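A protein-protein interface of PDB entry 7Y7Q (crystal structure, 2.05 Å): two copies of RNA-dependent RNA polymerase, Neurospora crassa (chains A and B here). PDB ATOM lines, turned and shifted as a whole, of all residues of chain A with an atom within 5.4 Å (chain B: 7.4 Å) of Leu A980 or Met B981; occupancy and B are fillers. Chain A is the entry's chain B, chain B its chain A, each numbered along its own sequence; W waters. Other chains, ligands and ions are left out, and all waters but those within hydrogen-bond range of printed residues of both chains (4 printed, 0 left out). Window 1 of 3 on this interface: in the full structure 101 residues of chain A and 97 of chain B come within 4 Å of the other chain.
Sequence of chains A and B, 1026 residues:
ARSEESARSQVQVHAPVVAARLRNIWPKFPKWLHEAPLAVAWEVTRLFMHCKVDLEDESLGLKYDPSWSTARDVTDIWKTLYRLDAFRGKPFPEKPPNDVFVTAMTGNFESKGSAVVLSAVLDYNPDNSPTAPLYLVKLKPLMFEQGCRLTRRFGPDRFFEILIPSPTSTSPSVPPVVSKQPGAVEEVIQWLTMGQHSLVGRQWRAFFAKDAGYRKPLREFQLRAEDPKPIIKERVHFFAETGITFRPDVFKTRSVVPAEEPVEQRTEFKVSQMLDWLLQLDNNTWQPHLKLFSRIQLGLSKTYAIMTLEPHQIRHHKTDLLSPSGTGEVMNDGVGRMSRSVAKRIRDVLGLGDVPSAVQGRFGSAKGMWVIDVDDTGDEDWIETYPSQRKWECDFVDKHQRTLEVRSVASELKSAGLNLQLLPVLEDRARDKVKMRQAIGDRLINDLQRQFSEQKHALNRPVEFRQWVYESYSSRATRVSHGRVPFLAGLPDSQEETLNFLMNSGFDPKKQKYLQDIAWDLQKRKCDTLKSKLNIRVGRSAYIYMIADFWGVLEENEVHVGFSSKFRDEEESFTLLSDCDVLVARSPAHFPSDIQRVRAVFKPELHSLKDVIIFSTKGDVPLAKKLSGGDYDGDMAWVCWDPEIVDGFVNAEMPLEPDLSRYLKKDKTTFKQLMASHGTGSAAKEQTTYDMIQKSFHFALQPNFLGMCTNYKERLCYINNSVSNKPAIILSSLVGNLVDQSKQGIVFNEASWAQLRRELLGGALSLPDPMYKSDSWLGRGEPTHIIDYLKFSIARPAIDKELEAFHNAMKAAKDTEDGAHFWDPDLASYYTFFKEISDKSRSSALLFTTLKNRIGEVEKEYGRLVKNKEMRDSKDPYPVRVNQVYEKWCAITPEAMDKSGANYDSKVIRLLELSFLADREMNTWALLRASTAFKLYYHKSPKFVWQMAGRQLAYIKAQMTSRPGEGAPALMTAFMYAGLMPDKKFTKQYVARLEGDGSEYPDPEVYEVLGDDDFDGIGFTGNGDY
O of Met A976 is in hydrogen-bond range of NH1 of Arg B466 (2.9 Å).
NH1 of Arg B476 is in salt-bridge range of OD2 of Asp A983 (3.1 Å).
O of Gly B979 sits at hydrogen-bond distance from N of Asp A983, 2.8 Å away.
O of Met A981 lies within hydrogen-bond range of N of Met B981, 2.8 Å away.
The backbone NH (N) of Asp B983 lies within hydrogen-bond range of the backbone carbonyl oxygen (O) of Gly A979 (2.8 Å).
The side-chain sulfur of Met A981 lies close to the side-chain carboxylate of Asp B983, 3.6 Å away.
The side-chain amide oxygen of Asn B504 lies within hydrogen-bond range of the guanidinium group of Arg B466, at 2.8 Å.
The backbone carbonyl oxygen (O) of Leu B980 sits at hydrogen-bond distance from the guanidinium group (NH1) of Arg B479 (3.1 Å).
The side-chain hydroxyl of Tyr B977 is in hydrogen-bond range of the side-chain amide nitrogen of Asn B504, at 2.9 Å.
The backbone carbonyl oxygen (O) of Ala A978 is in hydrogen-bond range of the guanidinium group (NH1) of Arg A479 (3.0 Å).
The backbone carbonyl oxygen of Leu A980 lies within hydrogen-bond range of the guanidinium group of Arg A479 (3.3 Å).
Among the printed residues, merely in contact across the chains: Asp A983 with Met B981, Met A972 with Asn B504, Met A981 with Leu B980, Leu A980 with Met B981, Gly A979 with Phe B986, Leu A980 with Arg B466, Met A976 with Asn B504, Pro A982 with Leu B980, Leu A980 with Pro B982, Met A972 with Tyr B977, Tyr A977 with Met B972, Ala A978 with Phe B986, Gly A979 with Arg B466, Pro A982 with Gly B979, Gly A979 with Pro B982, Met A972 with Met B972, Arg A479 with Phe B986 and Leu A980 with Leu B980.
Of the printed residues of chain B, Met A972 touches Asn B504 (3.4 Å), Met B972 (3.8 Å) and Tyr B977 (3.7 Å).
Of the printed residues of chain B, Met A976 touches Arg B466 and Asn B504.
Of the printed residues of chain B, Tyr A977 touches Met B972.
Of chain B, only Arg B466 (3.7 Å), Pro B982 (3.8 Å), Asp B983 (2.8 Å) and Phe B986 (3.5 Å) come within 4 Å of Gly A979.
Leu A980 touches just these residues of chain B: Arg B466 (3.5 Å), Leu B980 (3.96 Å), Met B981 (3.5 Å) and Pro B982 (3.7 Å).
Of the printed residues of chain A, Met B981 touches Leu A980 (3.5 Å), Met A981 (2.8 Å) and Asp A983 (3.2 Å).
Of the printed residues of chain A, Pro B982 touches Gly A979 (3.8 Å) and Leu A980 (3.7 Å).
The nearest residue of chain B that does not touch Leu A980 is Asp B983 (4.3 Å).
The nearest residue of chain A that does not touch Met B981 is Pro A982 (4.03 Å).
Of the 11 printed residues of chain A, 10 touch a printed residue of chain B.
Printed residues of chain A that touch a printed residue of chain B: Arg A479, Met A972, Met A976, Tyr A977, Ala A978, Gly A979, Leu A980, Met A981, Pro A982 and Asp A983.
Hydrophobic or aromatic side chains of chain A within 4 Å of the printed part of chain B: Met A972, Met A976, Tyr A977, Leu A980 and Met A981.
Of the 17 printed residues of chain B, 11 touch a printed residue of chain A.
Hydrophobic or aromatic side chains of chain B that line the printed part of chain A: Met B972, Tyr B977, Leu B980, Met B981 and Phe B986.
Among the printed residues, 24 pairs touch across the chains.
Among the printed residues, Asp or Glu carboxylates within 4 Å of a Lys or Arg side-chain nitrogen of the other chain: Asp A983 with Arg B476 (3.1 Å).
Met B972 touches its own counterpart, Met A972.
Met A972 touches Tyr B977, and with the chains exchanged Tyr A977 touches Met B972.
Leu A980 touches Pro B982, and with the chains exchanged Pro A982 touches Leu B980.
Met A981 touches its own counterpart, Met B981.
Positions printed for both chains: 479, 972, 976, 977, 978, 979, 980, 981, 982, 983 and 984.
Water W3 lies within hydrogen-bond range of O of Gly A979 (2.7 Å), NH2 of Arg B466 (3.1 Å) and O of Asp B983 (3.4 Å).
Water W1 bridges O of Gly B979 (2.8 Å) and O of Asp A983 (3.4 Å).
Water W4 bridges the guanidinium group of Arg B466 (2.9 Å) and the backbone NH of Gly A979 (3.4 Å).
Water W2 lies within hydrogen-bond range of OD2 of Asp A983 (2.9 Å), O of Ala B978 (3.2 Å) and NH1 of Arg B479 (3.4 Å).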
ATOM      1  N   ARG A 479      -7.162  -7.589   1.718  1.00  0.00           N
ATOM      2  CA  ARG A 479      -8.183  -8.032   0.773  1.00  0.00           C
ATOM      3  C   ARG A 479      -8.112  -7.238  -0.526  1.00  0.00           C
ATOM      4  O   ARG A 479      -8.204  -7.809  -1.618  1.00  0.00           O
ATOM      5  CB  ARG A 479      -9.572  -7.908   1.402  1.00  0.00           C
ATOM      6  CG  ARG A 479      -9.904  -9.000   2.409  1.00  0.00           C
ATOM      7  CD  ARG A 479     -11.067  -8.602   3.308  1.00  0.00           C
ATOM      8  NE  ARG A 479     -11.474  -9.698   4.180  1.00  0.00           N
ATOM      9  CZ  ARG A 479     -12.725 -10.113   4.338  1.00  0.00           C
ATOM     10  NH1 ARG A 479     -13.731  -9.539   3.698  1.00  0.00           N
ATOM     11  NH2 ARG A 479     -12.973 -11.129   5.159  1.00  0.00           N
ATOM     12  N   MET A 972     -20.061 -18.328  -2.567  1.00  0.00           N
ATOM     13  CA  MET A 972     -19.519 -17.031  -2.995  1.00  0.00           C
ATOM     14  C   MET A 972     -18.192 -17.216  -3.701  1.00  0.00           C
ATOM     15  O   MET A 972     -17.448 -18.094  -3.305  1.00  0.00           O
ATOM     16  CB  MET A 972     -19.266 -16.132  -1.789  1.00  0.00           C
ATOM     17  CG  MET A 972     -20.337 -16.214  -0.733  1.00  0.00           C
ATOM     18  SD  MET A 972     -21.258 -14.675  -0.643  1.00  0.00           S
ATOM     19  CE  MET A 972     -20.091 -13.549  -1.400  1.00  0.00           C
ATOM     20  N   MET A 976     -15.872 -11.920  -4.490  1.00  0.00           N
ATOM     21  CA  MET A 976     -17.134 -11.361  -3.948  1.00  0.00           C
ATOM     22  C   MET A 976     -17.177 -11.520  -2.423  1.00  0.00           C
ATOM     23  O   MET A 976     -17.692 -10.623  -1.770  1.00  0.00           O
ATOM     24  CB  MET A 976     -18.359 -11.954  -4.652  1.00  0.00           C
ATOM     25  CG  MET A 976     -18.469 -11.569  -6.119  1.00  0.00           C
ATOM     26  SD  MET A 976     -18.503  -9.787  -6.436  1.00  0.00           S
ATOM     27  CE  MET A 976     -20.264  -9.468  -6.389  1.00  0.00           C
ATOM     28  N   TYR A 977     -16.659 -12.626  -1.894  1.00  0.00           N
ATOM     29  CA  TYR A 977     -16.596 -12.842  -0.426  1.00  0.00           C
ATOM     30  C   TYR A 977     -15.712 -11.767   0.213  1.00  0.00           C
ATOM     31  O   TYR A 977     -16.045 -11.274   1.293  1.00  0.00           O
ATOM     32  CB  TYR A 977     -16.039 -14.237  -0.145  1.00  0.00           C
ATOM     33  CG  TYR A 977     -15.842 -14.608   1.300  1.00  0.00           C
ATOM     34  CD1 TYR A 977     -16.881 -15.126   2.048  1.00  0.00           C
ATOM     35  CD2 TYR A 977     -14.606 -14.477   1.908  1.00  0.00           C
ATOM     36  CE1 TYR A 977     -16.704 -15.491   3.371  1.00  0.00           C
ATOM     37  CE2 TYR A 977     -14.413 -14.832   3.231  1.00  0.00           C
ATOM     38  CZ  TYR A 977     -15.466 -15.343   3.964  1.00  0.00           C
ATOM     39  OH  TYR A 977     -15.293 -15.700   5.266  1.00  0.00           O
ATOM     40  N   ALA A 978     -14.619 -11.423  -0.453  1.00  0.00           N
ATOM     41  CA  ALA A 978     -13.652 -10.448   0.097  1.00  0.00           C
ATOM     42  C   ALA A 978     -14.259  -9.052   0.223  1.00  0.00           C
ATOM     43  O   ALA A 978     -13.756  -8.277   1.029  1.00  0.00           O
ATOM     44  CB  ALA A 978     -12.435 -10.430  -0.771  1.00  0.00           C
ATOM     45  N   GLY A 979     -15.278  -8.750  -0.573  1.00  0.00           N
ATOM     46  CA  GLY A 979     -15.861  -7.428  -0.533  1.00  0.00           C
ATOM     47  C   GLY A 979     -17.015  -7.257   0.430  1.00  0.00           C
ATOM     48  O   GLY A 979     -17.627  -6.183   0.451  1.00  0.00           O
ATOM     49  N   LEU A 980     -17.337  -8.273   1.222  1.00  0.00           N
ATOM     50  CA  LEU A 980     -18.412  -8.206   2.199  1.00  0.00           C
ATOM     51  C   LEU A 980     -17.851  -7.947   3.593  1.00  0.00           C
ATOM     52  O   LEU A 980     -16.658  -8.125   3.854  1.00  0.00           O
ATOM     53  CB  LEU A 980     -19.231  -9.500   2.194  1.00  0.00           C
ATOM     54  CG  LEU A 980     -20.024  -9.793   0.919  1.00  0.00           C
ATOM     55  CD1 LEU A 980     -20.996 -10.937   1.148  1.00  0.00           C
ATOM     56  CD2 LEU A 980     -20.765  -8.551   0.445  1.00  0.00           C
ATOM     57  N   MET A 981     -18.733  -7.516   4.490  1.00  0.00           N
ATOM     58  CA  MET A 981     -18.376  -7.220   5.870  1.00  0.00           C
ATOM     59  C   MET A 981     -19.596  -7.456   6.744  1.00  0.00           C
ATOM     60  O   MET A 981     -20.729  -7.373   6.256  1.00  0.00           O
ATOM     61  CB  MET A 981     -17.883  -5.775   6.034  1.00  0.00           C
ATOM     62  CG  MET A 981     -19.000  -4.746   6.016  1.00  0.00           C
ATOM     63  SD  MET A 981     -18.404  -3.059   6.210  1.00  0.00           S
ATOM     64  CE  MET A 981     -18.398  -2.911   7.996  1.00  0.00           C
ATOM     65  N   PRO A 982     -19.404  -7.757   8.027  1.00  0.00           N
ATOM     66  CA  PRO A 982     -20.559  -7.978   8.906  1.00  0.00           C
ATOM     67  C   PRO A 982     -21.424  -6.730   9.008  1.00  0.00           C
ATOM     68  O   PRO A 982     -20.924  -5.604   9.062  1.00  0.00           O
ATOM     69  CB  PRO A 982     -19.934  -8.338  10.260  1.00  0.00           C
ATOM     70  CG  PRO A 982     -18.464  -8.306  10.091  1.00  0.00           C
ATOM     71  CD  PRO A 982     -18.112  -8.056   8.667  1.00  0.00           C
ATOM     72  N   ASP A 983     -22.736  -6.947   9.027  1.00  0.00           N
ATOM     73  CA  ASP A 983     -23.718  -5.874   9.170  1.00  0.00           C
ATOM     74  C   ASP A 983     -23.926  -5.629  10.660  1.00  0.00           C
ATOM     75  O   ASP A 983     -24.598  -6.407  11.341  1.00  0.00           O
ATOM     76  CB  ASP A 983     -25.020  -6.250   8.471  1.00  0.00           C
ATOM     77  CG  ASP A 983     -26.091  -5.181   8.600  1.00  0.00           C
ATOM     78  OD1 ASP A 983     -25.836  -4.143   9.246  1.00  0.00           O
ATOM     79  OD2 ASP A 983     -27.192  -5.378   8.045  1.00  0.00           O
ATOM     80  N   LYS A 984     -23.349  -4.538  11.172  1.00  0.00           N
ATOM     81  CA  LYS A 984     -23.429  -4.264  12.604  1.00  0.00           C
ATOM     82  C   LYS A 984     -24.875  -4.148  13.072  1.00  0.00           C
ATOM     83  O   LYS A 984     -25.228  -4.649  14.146  1.00  0.00           O
ATOM     84  CB  LYS A 984     -22.650  -2.993  12.944  1.00  0.00           C
ATOM     85  CG  LYS A 984     -22.638  -2.646  14.430  1.00  0.00           C
ATOM     86  CD  LYS A 984     -21.924  -3.707  15.257  1.00  0.00           C
ATOM     87  CE  LYS A 984     -21.389  -3.122  16.558  1.00  0.00           C
ATOM     88  NZ  LYS A 984     -21.033  -4.175  17.550  1.00  0.00           N
ATOM     89  N   ARG B 466     -23.213  -4.392  -7.309  1.00  0.00           N
ATOM     90  CA  ARG B 466     -23.664  -4.876  -6.009  1.00  0.00           C
ATOM     91  C   ARG B 466     -23.779  -3.727  -5.017  1.00  0.00           C
ATOM     92  O   ARG B 466     -24.800  -3.577  -4.336  1.00  0.00           O
ATOM     93  CB  ARG B 466     -22.716  -5.954  -5.477  1.00  0.00           C
ATOM     94  CG  ARG B 466     -23.187  -6.567  -4.164  1.00  0.00           C
ATOM     95  CD  ARG B 466     -22.228  -7.620  -3.631  1.00  0.00           C
ATOM     96  NE  ARG B 466     -20.864  -7.129  -3.474  1.00  0.00           N
ATOM     97  CZ  ARG B 466     -19.838  -7.893  -3.124  1.00  0.00           C
ATOM     98  NH1 ARG B 466     -19.987  -9.187  -2.895  1.00  0.00           N
ATOM     99  NH2 ARG B 466     -18.632  -7.344  -3.003  1.00  0.00           N
ATOM    100  N   GLN B 467     -22.735  -2.903  -4.925  1.00  0.00           N
ATOM    101  CA  GLN B 467     -22.790  -1.725  -4.065  1.00  0.00           C
ATOM    102  C   GLN B 467     -24.003  -0.867  -4.400  1.00  0.00           C
ATOM    103  O   GLN B 467     -24.790  -0.502  -3.518  1.00  0.00           O
ATOM    104  CB  GLN B 467     -21.498  -0.918  -4.211  1.00  0.00           C
ATOM    105  CG  GLN B 467     -21.290   0.127  -3.137  1.00  0.00           C
ATOM    106  CD  GLN B 467     -21.128  -0.485  -1.764  1.00  0.00           C
ATOM    107  OE1 GLN B 467     -20.236  -1.302  -1.536  1.00  0.00           O
ATOM    108  NE2 GLN B 467     -21.995  -0.096  -0.840  1.00  0.00           N
ATOM    109  N   TYR B 470     -27.323  -2.500  -3.350  1.00  0.00           N
ATOM    110  CA  TYR B 470     -27.474  -2.520  -1.879  1.00  0.00           C
ATOM    111  C   TYR B 470     -27.963  -1.156  -1.391  1.00  0.00           C
ATOM    112  O   TYR B 470     -28.823  -1.101  -0.524  1.00  0.00           O
ATOM    113  CB  TYR B 470     -26.155  -2.873  -1.191  1.00  0.00           C
ATOM    114  CG  TYR B 470     -26.311  -2.878   0.303  1.00  0.00           C
ATOM    115  CD1 TYR B 470     -27.140  -3.806   0.902  1.00  0.00           C
ATOM    116  CD2 TYR B 470     -25.714  -1.916   1.098  1.00  0.00           C
ATOM    117  CE1 TYR B 470     -27.346  -3.811   2.267  1.00  0.00           C
ATOM    118  CE2 TYR B 470     -25.912  -1.904   2.466  1.00  0.00           C
ATOM    119  CZ  TYR B 470     -26.729  -2.855   3.047  1.00  0.00           C
ATOM    120  OH  TYR B 470     -26.960  -2.864   4.384  1.00  0.00           O
ATOM    121  N   ARG B 476     -32.694  -5.335   5.420  1.00  0.00           N
ATOM    122  CA  ARG B 476     -32.269  -5.748   6.752  1.00  0.00           C
ATOM    123  C   ARG B 476     -33.446  -6.242   7.585  1.00  0.00           C
ATOM    124  O   ARG B 476     -33.316  -7.210   8.343  1.00  0.00           O
ATOM    125  CB  ARG B 476     -31.558  -4.592   7.458  1.00  0.00           C
ATOM    126  CG  ARG B 476     -30.951  -4.966   8.799  1.00  0.00           C
ATOM    127  CD  ARG B 476     -29.839  -4.007   9.197  1.00  0.00           C
ATOM    128  NE  ARG B 476     -30.081  -2.654   8.710  1.00  0.00           N
ATOM    129  CZ  ARG B 476     -29.187  -1.917   8.064  1.00  0.00           C
ATOM    130  NH1 ARG B 476     -27.972  -2.372   7.807  1.00  0.00           N
ATOM    131  NH2 ARG B 476     -29.521  -0.693   7.669  1.00  0.00           N
ATOM    132  N   ARG B 479     -34.293  -9.840   6.541  1.00  0.00           N
ATOM    133  CA  ARG B 479     -33.219 -10.745   6.941  1.00  0.00           C
ATOM    134  C   ARG B 479     -33.239 -10.985   8.445  1.00  0.00           C
ATOM    135  O   ARG B 479     -33.072 -12.122   8.903  1.00  0.00           O
ATOM    136  CB  ARG B 479     -31.861 -10.194   6.495  1.00  0.00           C
ATOM    137  CG  ARG B 479     -31.702 -10.067   4.984  1.00  0.00           C
ATOM    138  CD  ARG B 479     -30.452  -9.286   4.599  1.00  0.00           C
ATOM    139  NE  ARG B 479     -30.014  -9.631   3.250  1.00  0.00           N
ATOM    140  CZ  ARG B 479     -28.748  -9.761   2.875  1.00  0.00           C
ATOM    141  NH1 ARG B 479     -27.751  -9.591   3.728  1.00  0.00           N
ATOM    142  NH2 ARG B 479     -28.476 -10.072   1.611  1.00  0.00           N
ATOM    143  N   ASN B 504     -22.984 -12.548  -6.453  1.00  0.00           N
ATOM    144  CA  ASN B 504     -22.057 -13.107  -5.476  1.00  0.00           C
ATOM    145  C   ASN B 504     -21.538 -14.478  -5.893  1.00  0.00           C
ATOM    146  O   ASN B 504     -20.479 -14.898  -5.415  1.00  0.00           O
ATOM    147  CB  ASN B 504     -22.724 -13.186  -4.101  1.00  0.00           C
ATOM    148  CG  ASN B 504     -22.753 -11.845  -3.392  1.00  0.00           C
ATOM    149  OD1 ASN B 504     -21.937 -10.965  -3.673  1.00  0.00           O
ATOM    150  ND2 ASN B 504     -23.691 -11.682  -2.467  1.00  0.00           N
ATOM    151  N   MET B 972     -21.340 -20.357   2.273  1.00  0.00           N
ATOM    152  CA  MET B 972     -21.852 -19.752   3.511  1.00  0.00           C
ATOM    153  C   MET B 972     -23.230 -20.302   3.846  1.00  0.00           C
ATOM    154  O   MET B 972     -23.959 -20.624   2.922  1.00  0.00           O
ATOM    155  CB  MET B 972     -21.938 -18.234   3.358  1.00  0.00           C
ATOM    156  CG  MET B 972     -20.691 -17.624   2.777  1.00  0.00           C
ATOM    157  SD  MET B 972     -20.359 -16.030   3.533  1.00  0.00           S
ATOM    158  CE  MET B 972     -21.859 -15.158   3.095  1.00  0.00           C
ATOM    159  N   MET B 976     -25.604 -16.981   8.075  1.00  0.00           N
ATOM    160  CA  MET B 976     -24.354 -16.184   8.008  1.00  0.00           C
ATOM    161  C   MET B 976     -24.340 -15.303   6.758  1.00  0.00           C
ATOM    162  O   MET B 976     -23.854 -14.175   6.855  1.00  0.00           O
ATOM    163  CB  MET B 976     -23.119 -17.085   8.059  1.00  0.00           C
ATOM    164  CG  MET B 976     -22.918 -17.775   9.401  1.00  0.00           C
ATOM    165  SD  MET B 976     -23.046 -16.692  10.849  1.00  0.00           S
ATOM    166  CE  MET B 976     -21.316 -16.360  11.170  1.00  0.00           C
ATOM    167  N   TYR B 977     -24.907 -15.746   5.637  1.00  0.00           N
ATOM    168  CA  TYR B 977     -24.994 -14.884   4.428  1.00  0.00           C
ATOM    169  C   TYR B 977     -25.863 -13.657   4.713  1.00  0.00           C
ATOM    170  O   TYR B 977     -25.494 -12.561   4.291  1.00  0.00           O
ATOM    171  CB  TYR B 977     -25.533 -15.670   3.231  1.00  0.00           C
ATOM    172  CG  TYR B 977     -25.728 -14.898   1.953  1.00  0.00           C
ATOM    173  CD1 TYR B 977     -24.662 -14.631   1.115  1.00  0.00           C
ATOM    174  CD2 TYR B 977     -26.983 -14.466   1.560  1.00  0.00           C
ATOM    175  CE1 TYR B 977     -24.829 -13.941  -0.072  1.00  0.00           C
ATOM    176  CE2 TYR B 977     -27.168 -13.772   0.379  1.00  0.00           C
ATOM    177  CZ  TYR B 977     -26.087 -13.511  -0.443  1.00  0.00           C
ATOM    178  OH  TYR B 977     -26.253 -12.831  -1.611  1.00  0.00           O
ATOM    179  N   ALA B 978     -26.948 -13.849   5.447  1.00  0.00           N
ATOM    180  CA  ALA B 978     -27.897 -12.757   5.737  1.00  0.00           C
ATOM    181  C   ALA B 978     -27.252 -11.651   6.572  1.00  0.00           C
ATOM    182  O   ALA B 978     -27.707 -10.509   6.466  1.00  0.00           O
ATOM    183  CB  ALA B 978     -29.115 -13.327   6.396  1.00  0.00           C
ATOM    184  N   GLY B 979     -26.254 -11.976   7.386  1.00  0.00           N
ATOM    185  CA  GLY B 979     -25.667 -10.980   8.298  1.00  0.00           C
ATOM    186  C   GLY B 979     -24.601 -10.131   7.661  1.00  0.00           C
ATOM    187  O   GLY B 979     -24.037  -9.300   8.359  1.00  0.00           O
ATOM    188  N   LEU B 980     -24.319 -10.353   6.386  1.00  0.00           N
ATOM    189  CA  LEU B 980     -23.224  -9.630   5.698  1.00  0.00           C
ATOM    190  C   LEU B 980     -23.772  -8.522   4.799  1.00  0.00           C
ATOM    191  O   LEU B 980     -24.908  -8.638   4.340  1.00  0.00           O
ATOM    192  CB  LEU B 980     -22.377 -10.624   4.902  1.00  0.00           C
ATOM    193  CG  LEU B 980     -21.570 -11.631   5.716  1.00  0.00           C
ATOM    194  CD1 LEU B 980     -20.568 -12.345   4.829  1.00  0.00           C
ATOM    195  CD2 LEU B 980     -20.852 -10.952   6.864  1.00  0.00           C
ATOM    196  N   MET B 981     -22.974  -7.477   4.640  1.00  0.00           N
ATOM    197  CA  MET B 981     -23.346  -6.333   3.796  1.00  0.00           C
ATOM    198  C   MET B 981     -22.139  -5.963   2.922  1.00  0.00           C
ATOM    199  O   MET B 981     -21.016  -6.244   3.340  1.00  0.00           O
ATOM    200  CB  MET B 981     -23.757  -5.117   4.634  1.00  0.00           C
ATOM    201  CG  MET B 981     -22.683  -4.625   5.575  1.00  0.00           C
ATOM    202  SD  MET B 981     -22.888  -2.890   6.029  1.00  0.00           S
ATOM    203  CE  MET B 981     -24.595  -2.886   6.558  1.00  0.00           C
ATOM    204  N   PRO B 982     -22.312  -5.374   1.717  1.00  0.00           N
ATOM    205  CA  PRO B 982     -21.178  -4.919   0.927  1.00  0.00           C
ATOM    206  C   PRO B 982     -20.339  -3.886   1.686  1.00  0.00           C
ATOM    207  O   PRO B 982     -20.904  -3.093   2.391  1.00  0.00           O
ATOM    208  CB  PRO B 982     -21.861  -4.255  -0.268  1.00  0.00           C
ATOM    209  CG  PRO B 982     -23.173  -4.975  -0.393  1.00  0.00           C
ATOM    210  CD  PRO B 982     -23.594  -5.181   1.042  1.00  0.00           C
ATOM    211  N   ASP B 983     -19.017  -3.954   1.544  1.00  0.00           N
ATOM    212  CA  ASP B 983     -18.102  -2.992   2.208  1.00  0.00           C
ATOM    213  C   ASP B 983     -17.817  -1.861   1.229  1.00  0.00           C
ATOM    214  O   ASP B 983     -17.028  -2.068   0.298  1.00  0.00           O
ATOM    215  CB  ASP B 983     -16.805  -3.686   2.616  1.00  0.00           C
ATOM    216  CG  ASP B 983     -15.815  -2.829   3.382  1.00  0.00           C
ATOM    217  OD1 ASP B 983     -16.170  -1.701   3.763  1.00  0.00           O
ATOM    218  OD2 ASP B 983     -14.694  -3.310   3.595  1.00  0.00           O
ATOM    219  N   LYS B 984     -18.419  -0.700   1.470  1.00  0.00           N
ATOM    220  CA  LYS B 984     -18.239   0.454   0.555  1.00  0.00           C
ATOM    221  C   LYS B 984     -16.752   0.808   0.504  1.00  0.00           C
ATOM    222  O   LYS B 984     -16.268   1.128  -0.582  1.00  0.00           O
ATOM    223  CB  LYS B 984     -19.136   1.605   1.005  1.00  0.00           C
ATOM    224  CG  LYS B 984     -18.986   2.906   0.230  1.00  0.00           C
ATOM    225  CD  LYS B 984     -19.514   2.830  -1.184  1.00  0.00           C
ATOM    226  CE  LYS B 984     -19.941   4.176  -1.730  1.00  0.00           C
ATOM    227  NZ  LYS B 984     -20.647   4.043  -3.027  1.00  0.00           N
ATOM    228  N   PHE B 986     -14.173  -1.160   0.714  1.00  0.00           N
ATOM    229  CA  PHE B 986     -13.519  -2.108  -0.182  1.00  0.00           C
ATOM    230  C   PHE B 986     -13.787  -1.753  -1.639  1.00  0.00           C
ATOM    231  O   PHE B 986     -12.874  -1.766  -2.473  1.00  0.00           O
ATOM    232  CB  PHE B 986     -13.987  -3.534   0.117  1.00  0.00           C
ATOM    233  CG  PHE B 986     -13.450  -4.562  -0.844  1.00  0.00           C
ATOM    234  CD1 PHE B 986     -14.101  -4.823  -2.041  1.00  0.00           C
ATOM    235  CD2 PHE B 986     -12.292  -5.265  -0.554  1.00  0.00           C
ATOM    236  CE1 PHE B 986     -13.607  -5.763  -2.929  1.00  0.00           C
ATOM    237  CE2 PHE B 986     -11.793  -6.208  -1.436  1.00  0.00           C
ATOM    238  CZ  PHE B 986     -12.453  -6.458  -2.624  1.00  0.00           C
HETATM  239  O   HOH W   1     -23.704  -9.668  11.150  1.00  0.00           O
HETATM  240  O   HOH W   2     -28.285  -7.407   6.222  1.00  0.00           O
HETATM  241  O   HOH W   3     -17.698  -4.656  -1.832  1.00  0.00           O
HETATM  242  O   HOH W   4     -16.033  -8.193  -3.872  1.00  0.00           O
